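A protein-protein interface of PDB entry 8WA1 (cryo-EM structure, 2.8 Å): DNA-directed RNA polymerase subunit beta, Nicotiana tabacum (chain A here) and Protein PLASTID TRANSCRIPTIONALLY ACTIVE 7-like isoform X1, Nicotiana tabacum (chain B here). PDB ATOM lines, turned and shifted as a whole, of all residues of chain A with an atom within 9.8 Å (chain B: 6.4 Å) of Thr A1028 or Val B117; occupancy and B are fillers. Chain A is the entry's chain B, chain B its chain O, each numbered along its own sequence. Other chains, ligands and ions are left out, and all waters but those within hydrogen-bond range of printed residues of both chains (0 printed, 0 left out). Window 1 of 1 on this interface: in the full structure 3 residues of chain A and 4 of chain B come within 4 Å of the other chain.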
ATOM      1  N   TYR A1008     -18.462  31.966  11.954  1.00  0.00           N
ATOM      2  CA  TYR A1008     -19.002  30.760  11.326  1.00  0.00           C
ATOM      3  C   TYR A1008     -20.411  30.446  11.810  1.00  0.00           C
ATOM      4  O   TYR A1008     -21.162  29.745  11.124  1.00  0.00           O
ATOM      5  CB  TYR A1008     -18.057  29.563  11.504  1.00  0.00           C
ATOM      6  CG  TYR A1008     -17.817  29.002  12.891  1.00  0.00           C
ATOM      7  CD1 TYR A1008     -18.840  28.414  13.624  1.00  0.00           C
ATOM      8  CD2 TYR A1008     -16.539  28.998  13.436  1.00  0.00           C
ATOM      9  CE1 TYR A1008     -18.606  27.879  14.879  1.00  0.00           C
ATOM     10  CE2 TYR A1008     -16.294  28.459  14.682  1.00  0.00           C
ATOM     11  CZ  TYR A1008     -17.330  27.903  15.400  1.00  0.00           C
ATOM     12  OH  TYR A1008     -17.088  27.373  16.646  1.00  0.00           O
ATOM     13  N   ALA A1015     -16.996  28.293   6.176  1.00  0.00           N
ATOM     14  CA  ALA A1015     -16.767  27.713   7.462  1.00  0.00           C
ATOM     15  C   ALA A1015     -18.050  27.067   7.901  1.00  0.00           C
ATOM     16  O   ALA A1015     -18.033  25.968   8.430  1.00  0.00           O
ATOM     17  CB  ALA A1015     -16.320  28.758   8.436  1.00  0.00           C
ATOM     18  N   GLU A1018     -18.575  23.856   6.454  1.00  0.00           N
ATOM     19  CA  GLU A1018     -17.670  22.826   6.956  1.00  0.00           C
ATOM     20  C   GLU A1018     -18.020  22.425   8.384  1.00  0.00           C
ATOM     21  O   GLU A1018     -17.639  21.341   8.840  1.00  0.00           O
ATOM     22  CB  GLU A1018     -16.221  23.312   6.890  1.00  0.00           C
ATOM     23  CG  GLU A1018     -15.700  23.599   5.493  1.00  0.00           C
ATOM     24  CD  GLU A1018     -14.290  24.159   5.514  1.00  0.00           C
ATOM     25  OE1 GLU A1018     -13.485  23.780   4.639  1.00  0.00           O
ATOM     26  OE2 GLU A1018     -13.988  24.973   6.412  1.00  0.00           O
ATOM     27  N   VAL A1019     -18.720  23.301   9.111  1.00  0.00           N
ATOM     28  CA  VAL A1019     -19.039  23.029  10.512  1.00  0.00           C
ATOM     29  C   VAL A1019     -19.920  21.792  10.640  1.00  0.00           C
ATOM     30  O   VAL A1019     -19.692  20.939  11.504  1.00  0.00           O
ATOM     31  CB  VAL A1019     -19.689  24.267  11.160  1.00  0.00           C
ATOM     32  CG1 VAL A1019     -20.723  23.856  12.202  1.00  0.00           C
ATOM     33  CG2 VAL A1019     -18.627  25.150  11.798  1.00  0.00           C
ATOM     34  N   GLY A1021     -20.197  19.237   8.565  1.00  0.00           N
ATOM     35  CA  GLY A1021     -19.412  18.050   8.269  1.00  0.00           C
ATOM     36  C   GLY A1021     -18.476  17.675   9.402  1.00  0.00           C
ATOM     37  O   GLY A1021     -18.366  16.503   9.772  1.00  0.00           O
ATOM     38  N   THR A1022     -17.795  18.671   9.976  1.00  0.00           N
ATOM     39  CA  THR A1022     -16.857  18.393  11.059  1.00  0.00           C
ATOM     40  C   THR A1022     -17.580  17.907  12.308  1.00  0.00           C
ATOM     41  O   THR A1022     -17.042  17.092  13.067  1.00  0.00           O
ATOM     42  CB  THR A1022     -16.026  19.639  11.373  1.00  0.00           C
ATOM     43  OG1 THR A1022     -16.896  20.761  11.568  1.00  0.00           O
ATOM     44  CG2 THR A1022     -15.060  19.937  10.236  1.00  0.00           C
ATOM     45  N   THR A1023     -18.799  18.396  12.543  1.00  0.00           N
ATOM     46  CA  THR A1023     -19.555  17.956  13.710  1.00  0.00           C
ATOM     47  C   THR A1023     -20.106  16.550  13.510  1.00  0.00           C
ATOM     48  O   THR A1023     -20.116  15.744  14.448  1.00  0.00           O
ATOM     49  CB  THR A1023     -20.684  18.939  14.010  1.00  0.00           C
ATOM     50  OG1 THR A1023     -20.190  20.281  13.920  1.00  0.00           O
ATOM     51  CG2 THR A1023     -21.229  18.707  15.411  1.00  0.00           C
ATOM     52  N   ILE A1024     -20.573  16.239  12.299  1.00  0.00           N
ATOM     53  CA  ILE A1024     -21.089  14.901  12.025  1.00  0.00           C
ATOM     54  C   ILE A1024     -19.965  13.872  12.072  1.00  0.00           C
ATOM     55  O   ILE A1024     -20.123  12.786  12.644  1.00  0.00           O
ATOM     56  CB  ILE A1024     -21.826  14.882  10.674  1.00  0.00           C
ATOM     57  CG1 ILE A1024     -23.123  15.690  10.765  1.00  0.00           C
ATOM     58  CG2 ILE A1024     -22.115  13.454  10.236  1.00  0.00           C
ATOM     59  CD1 ILE A1024     -23.875  15.787   9.457  1.00  0.00           C
ATOM     60  N   ILE A1025     -18.812  14.195  11.483  1.00  0.00           N
ATOM     61  CA  ILE A1025     -17.676  13.278  11.534  1.00  0.00           C
ATOM     62  C   ILE A1025     -17.091  13.235  12.941  1.00  0.00           C
ATOM     63  O   ILE A1025     -16.718  12.168  13.443  1.00  0.00           O
ATOM     64  CB  ILE A1025     -16.618  13.676  10.489  1.00  0.00           C
ATOM     65  CG1 ILE A1025     -17.200  13.580   9.079  1.00  0.00           C
ATOM     66  CG2 ILE A1025     -15.380  12.799  10.615  1.00  0.00           C
ATOM     67  CD1 ILE A1025     -16.255  14.051   7.995  1.00  0.00           C
ATOM     68  N   GLY A1026     -17.013  14.389  13.601  1.00  0.00           N
ATOM     69  CA  GLY A1026     -16.453  14.482  14.933  1.00  0.00           C
ATOM     70  C   GLY A1026     -15.097  15.147  15.016  1.00  0.00           C
ATOM     71  O   GLY A1026     -14.531  15.221  16.113  1.00  0.00           O
ATOM     72  N   GLY A1027     -14.560  15.634  13.899  1.00  0.00           N
ATOM     73  CA  GLY A1027     -13.256  16.260  13.923  1.00  0.00           C
ATOM     74  C   GLY A1027     -13.287  17.652  14.524  1.00  0.00           C
ATOM     75  O   GLY A1027     -14.336  18.272  14.692  1.00  0.00           O
ATOM     76  N   THR A1028     -12.097  18.144  14.858  1.00  0.00           N
ATOM     77  CA  THR A1028     -11.970  19.479  15.424  1.00  0.00           C
ATOM     78  C   THR A1028     -12.230  20.535  14.355  1.00  0.00           C
ATOM     79  O   THR A1028     -11.823  20.386  13.199  1.00  0.00           O
ATOM     80  CB  THR A1028     -10.577  19.668  16.028  1.00  0.00           C
ATOM     81  OG1 THR A1028     -10.297  18.593  16.934  1.00  0.00           O
ATOM     82  CG2 THR A1028     -10.490  20.988  16.784  1.00  0.00           C
ATOM     83  N   ILE A1029     -12.911  21.604  14.747  1.00  0.00           N
ATOM     84  CA  ILE A1029     -13.273  22.684  13.834  1.00  0.00           C
ATOM     85  C   ILE A1029     -12.093  23.649  13.753  1.00  0.00           C
ATOM     86  O   ILE A1029     -11.707  24.220  14.784  1.00  0.00           O
ATOM     87  CB  ILE A1029     -14.541  23.409  14.297  1.00  0.00           C
ATOM     88  CG1 ILE A1029     -15.719  22.434  14.361  1.00  0.00           C
ATOM     89  CG2 ILE A1029     -14.857  24.574  13.371  1.00  0.00           C
ATOM     90  CD1 ILE A1029     -17.011  23.069  14.823  1.00  0.00           C
ATOM     91  N   PRO A1030     -11.504  23.858  12.578  1.00  0.00           N
ATOM     92  CA  PRO A1030     -10.375  24.787  12.478  1.00  0.00           C
ATOM     93  C   PRO A1030     -10.826  26.232  12.610  1.00  0.00           C
ATOM     94  O   PRO A1030     -11.981  26.577  12.353  1.00  0.00           O
ATOM     95  CB  PRO A1030      -9.812  24.506  11.081  1.00  0.00           C
ATOM     96  CG  PRO A1030     -10.992  24.021  10.305  1.00  0.00           C
ATOM     97  CD  PRO A1030     -11.839  23.246  11.280  1.00  0.00           C
ATOM     98  N   ASN A1031      -9.890  27.082  13.016  1.00  0.00           N
ATOM     99  CA  ASN A1031     -10.186  28.500  13.173  1.00  0.00           C
ATOM    100  C   ASN A1031     -10.241  29.173  11.804  1.00  0.00           C
ATOM    101  O   ASN A1031      -9.287  29.060  11.028  1.00  0.00           O
ATOM    102  CB  ASN A1031      -9.134  29.176  14.047  1.00  0.00           C
ATOM    103  CG  ASN A1031      -9.088  28.605  15.450  1.00  0.00           C
ATOM    104  OD1 ASN A1031      -9.558  27.495  15.696  1.00  0.00           O
ATOM    105  ND2 ASN A1031      -8.521  29.365  16.380  1.00  0.00           N
ATOM    106  N   PRO A1032     -11.328  29.869  11.477  1.00  0.00           N
ATOM    107  CA  PRO A1032     -11.417  30.516  10.162  1.00  0.00           C
ATOM    108  C   PRO A1032     -10.402  31.642  10.029  1.00  0.00           C
ATOM    109  O   PRO A1032     -10.186  32.423  10.958  1.00  0.00           O
ATOM    110  CB  PRO A1032     -12.854  31.049  10.125  1.00  0.00           C
ATOM    111  CG  PRO A1032     -13.588  30.278  11.185  1.00  0.00           C
ATOM    112  CD  PRO A1032     -12.573  30.008  12.248  1.00  0.00           C
ATOM    113  N   GLU B 112      -4.456  20.658  24.379  1.00  0.00           N
ATOM    114  CA  GLU B 112      -4.381  19.264  24.809  1.00  0.00           C
ATOM    115  C   GLU B 112      -5.651  18.504  24.445  1.00  0.00           C
ATOM    116  O   GLU B 112      -5.587  17.344  24.017  1.00  0.00           O
ATOM    117  CB  GLU B 112      -4.117  19.194  26.312  1.00  0.00           C
ATOM    118  CG  GLU B 112      -3.785  17.800  26.815  1.00  0.00           C
ATOM    119  CD  GLU B 112      -3.268  17.803  28.241  1.00  0.00           C
ATOM    120  OE1 GLU B 112      -3.172  18.896  28.837  1.00  0.00           O
ATOM    121  OE2 GLU B 112      -2.954  16.713  28.764  1.00  0.00           O
ATOM    122  N   ALA B 113      -6.814  19.142  24.594  1.00  0.00           N
ATOM    123  CA  ALA B 113      -8.062  18.504  24.193  1.00  0.00           C
ATOM    124  C   ALA B 113      -8.129  18.307  22.686  1.00  0.00           C
ATOM    125  O   ALA B 113      -8.657  17.292  22.217  1.00  0.00           O
ATOM    126  CB  ALA B 113      -9.255  19.331  24.673  1.00  0.00           C
ATOM    127  N   LYS B 114      -7.593  19.254  21.911  1.00  0.00           N
ATOM    128  CA  LYS B 114      -7.539  19.080  20.464  1.00  0.00           C
ATOM    129  C   LYS B 114      -6.656  17.898  20.090  1.00  0.00           C
ATOM    130  O   LYS B 114      -7.005  17.110  19.203  1.00  0.00           O
ATOM    131  CB  LYS B 114      -7.034  20.363  19.800  1.00  0.00           C
ATOM    132  CG  LYS B 114      -6.873  20.263  18.291  1.00  0.00           C
ATOM    133  CD  LYS B 114      -6.346  21.565  17.709  1.00  0.00           C
ATOM    134  CE  LYS B 114      -6.096  21.444  16.214  1.00  0.00           C
ATOM    135  NZ  LYS B 114      -7.339  21.119  15.462  1.00  0.00           N
ATOM    136  N   GLN B 115      -5.508  17.759  20.756  1.00  0.00           N
ATOM    137  CA  GLN B 115      -4.654  16.599  20.511  1.00  0.00           C
ATOM    138  C   GLN B 115      -5.367  15.302  20.873  1.00  0.00           C
ATOM    139  O   GLN B 115      -5.293  14.315  20.130  1.00  0.00           O
ATOM    140  CB  GLN B 115      -3.346  16.727  21.292  1.00  0.00           C
ATOM    141  CG  GLN B 115      -2.336  17.675  20.666  1.00  0.00           C
ATOM    142  CD  GLN B 115      -0.999  17.657  21.383  1.00  0.00           C
ATOM    143  OE1 GLN B 115      -0.030  18.265  20.929  1.00  0.00           O
ATOM    144  NE2 GLN B 115      -0.941  16.958  22.511  1.00  0.00           N
ATOM    145  N   TYR B 116      -6.064  15.283  22.013  1.00  0.00           N
ATOM    146  CA  TYR B 116      -6.804  14.088  22.412  1.00  0.00           C
ATOM    147  C   TYR B 116      -7.871  13.725  21.385  1.00  0.00           C
ATOM    148  O   TYR B 116      -8.058  12.546  21.063  1.00  0.00           O
ATOM    149  CB  TYR B 116      -7.439  14.288  23.789  1.00  0.00           C
ATOM    150  CG  TYR B 116      -6.502  14.048  24.951  1.00  0.00           C
ATOM    151  CD1 TYR B 116      -5.127  14.004  24.765  1.00  0.00           C
ATOM    152  CD2 TYR B 116      -6.996  13.872  26.236  1.00  0.00           C
ATOM    153  CE1 TYR B 116      -4.271  13.786  25.829  1.00  0.00           C
ATOM    154  CE2 TYR B 116      -6.148  13.653  27.304  1.00  0.00           C
ATOM    155  CZ  TYR B 116      -4.787  13.612  27.095  1.00  0.00           C
ATOM    156  OH  TYR B 116      -3.939  13.396  28.157  1.00  0.00           O
ATOM    157  N   VAL B 117      -8.587  14.726  20.869  1.00  0.00           N
ATOM    158  CA  VAL B 117      -9.622  14.462  19.874  1.00  0.00           C
ATOM    159  C   VAL B 117      -9.004  13.950  18.580  1.00  0.00           C
ATOM    160  O   VAL B 117      -9.507  13.000  17.968  1.00  0.00           O
ATOM    161  CB  VAL B 117     -10.469  15.728  19.639  1.00  0.00           C
ATOM    162  CG1 VAL B 117     -11.328  15.573  18.394  1.00  0.00           C
ATOM    163  CG2 VAL B 117     -11.339  16.009  20.851  1.00  0.00           C
ATOM    164  N   GLU B 118      -7.897  14.559  18.146  1.00  0.00           N
ATOM    165  CA  GLU B 118      -7.258  14.135  16.905  1.00  0.00           C
ATOM    166  C   GLU B 118      -6.683  12.730  17.027  1.00  0.00           C
ATOM    167  O   GLU B 118      -6.596  11.999  16.033  1.00  0.00           O
ATOM    168  CB  GLU B 118      -6.166  15.130  16.509  1.00  0.00           C
ATOM    169  CG  GLU B 118      -6.470  15.918  15.244  1.00  0.00           C
ATOM    170  CD  GLU B 118      -7.661  16.845  15.399  1.00  0.00           C
ATOM    171  OE1 GLU B 118      -7.950  17.263  16.539  1.00  0.00           O
ATOM    172  OE2 GLU B 118      -8.307  17.157  14.377  1.00  0.00           O
ATOM    173  N   ASN B 119      -6.281  12.334  18.235  1.00  0.00           N
ATOM    174  CA  ASN B 119      -5.720  10.998  18.418  1.00  0.00           C
ATOM    175  C   ASN B 119      -6.797   9.925  18.304  1.00  0.00           C
ATOM    176  O   ASN B 119      -6.605   8.912  17.620  1.00  0.00           O
ATOM    177  CB  ASN B 119      -5.004  10.910  19.767  1.00  0.00           C
ATOM    178  CG  ASN B 119      -3.723  11.724  19.802  1.00  0.00           C
ATOM    179  OD1 ASN B 119      -3.085  11.938  18.772  1.00  0.00           O
ATOM    180  ND2 ASN B 119      -3.345  12.183  20.990  1.00  0.00           N
ATOM    181  N   ASN B 120      -7.941  10.127  18.966  1.00  0.00           N
ATOM    182  CA  ASN B 120      -9.028   9.147  18.989  1.00  0.00           C
ATOM    183  C   ASN B 120     -10.364   9.875  18.821  1.00  0.00           C
ATOM    184  O   ASN B 120     -10.924  10.417  19.775  1.00  0.00           O
ATOM    185  CB  ASN B 120      -8.995   8.323  20.278  1.00  0.00           C
ATOM    186  CG  ASN B 120      -7.744   7.479  20.396  1.00  0.00           C
ATOM    187  OD1 ASN B 120      -6.957   7.640  21.328  1.00  0.00           O
ATOM    188  ND2 ASN B 120      -7.553   6.568  19.448  1.00  0.00           N
ATOM    189  N   ARG B 121     -10.878   9.881  17.588  1.00  0.00           N
ATOM    190  CA  ARG B 121     -12.157  10.535  17.322  1.00  0.00           C
ATOM    191  C   ARG B 121     -13.320   9.722  17.880  1.00  0.00           C
ATOM    192  O   ARG B 121     -14.182  10.254  18.590  1.00  0.00           O
ATOM    193  CB  ARG B 121     -12.329  10.762  15.821  1.00  0.00           C
ATOM    194  CG  ARG B 121     -11.399  11.812  15.239  1.00  0.00           C
ATOM    195  CD  ARG B 121     -11.720  12.092  13.779  1.00  0.00           C
ATOM    196  NE  ARG B 121     -10.857  13.131  13.224  1.00  0.00           N
ATOM    197  CZ  ARG B 121     -10.923  13.571  11.972  1.00  0.00           C
ATOM    198  NH1 ARG B 121     -11.816  13.064  11.133  1.00  0.00           N
ATOM    199  NH2 ARG B 121     -10.095  14.520  11.557  1.00  0.00           N
ATOM    200  N   ASP B 122     -13.361   8.425  17.565  1.00  0.00           N
ATOM    201  CA  ASP B 122     -14.503   7.601  17.951  1.00  0.00           C
ATOM    202  C   ASP B 122     -14.599   7.428  19.461  1.00  0.00           C
ATOM    203  O   ASP B 122     -15.668   7.083  19.978  1.00  0.00           O
ATOM    204  CB  ASP B 122     -14.421   6.234  17.268  1.00  0.00           C
ATOM    205  N   TYR B 124     -14.543   9.720  21.740  1.00  0.00           N
ATOM    206  CA  TYR B 124     -15.385  10.758  22.309  1.00  0.00           C
ATOM    207  C   TYR B 124     -16.701  10.876  21.542  1.00  0.00           C
ATOM    208  O   TYR B 124     -16.891  10.281  20.479  1.00  0.00           O
ATOM    209  CB  TYR B 124     -14.646  12.097  22.316  1.00  0.00           C
ATOM    210  CG  TYR B 124     -13.277  12.017  22.951  1.00  0.00           C
ATOM    211  CD1 TYR B 124     -13.136  11.879  24.327  1.00  0.00           C
ATOM    212  CD2 TYR B 124     -12.128  12.072  22.178  1.00  0.00           C
ATOM    213  CE1 TYR B 124     -11.886  11.800  24.913  1.00  0.00           C
ATOM    214  CE2 TYR B 124     -10.872  11.995  22.756  1.00  0.00           C
ATOM    215  CZ  TYR B 124     -10.758  11.859  24.123  1.00  0.00           C
ATOM    216  OH  TYR B 124      -9.514  11.783  24.703  1.00  0.00           O
ATOM    217  N   ALA B 129     -13.553  15.405  25.898  1.00  0.00           N
ATOM    218  CA  ALA B 129     -12.094  15.397  25.894  1.00  0.00           C
ATOM    219  C   ALA B 129     -11.533  16.385  26.908  1.00  0.00           C
ATOM    220  O   ALA B 129     -10.482  16.140  27.507  1.00  0.00           O
ATOM    221  CB  ALA B 129     -11.573  15.710  24.493  1.00  0.00           C
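Among the printed residues, pairs that only touch across the chains: Ile A1025 with Arg B121 (3.6 Å), Gly A1026 with Val B117 (3.9 Å), Thr A1028 with Lys B114 (3.4 Å) and Thr A1028 with Val B117 (3.5 Å).
Of the printed residues of chain B, Ile A1025 touches Arg B121. Of the printed residues of chain B, Gly A1026 touches Val B117 (3.9 Å). Thr A1028 touches three residues of chain B. Glu B112 touches none of the printed residues of chain A. Val B117 touches just these residues of chain A: Gly A1026 (3.9 Å) and Thr A1028 (3.5 Å). Of the printed residues of chain A, Arg B121 touches Ile A1025 (3.6 Å). The nearest residue of chain B that does not touch Thr A1028 is Arg B121 (5.3 Å). The nearest residue of chain A that does not touch Val B117 is Gly A1027 (4.8 Å). The nearest printed residue of chain B that does not touch Ile A1025 is Asp B122 (6.5 Å).
Of the 16 printed residues of chain A, 3 touch a printed residue of chain B. Of the 13 printed residues of chain B, 4 touch a printed residue of chain A. Hydrophobic or aromatic side chains of chain B within 4 Å of the printed part of chain A: Val B117. Along chain B the printed residues that touch a printed residue of chain A span positions 114 to 121. Among the printed residues, 5 pairs touch across the chains.
OG1 of Thr A1028 lies within hydrogen-bond range of OE1 of Glu B118 (2.7 Å).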
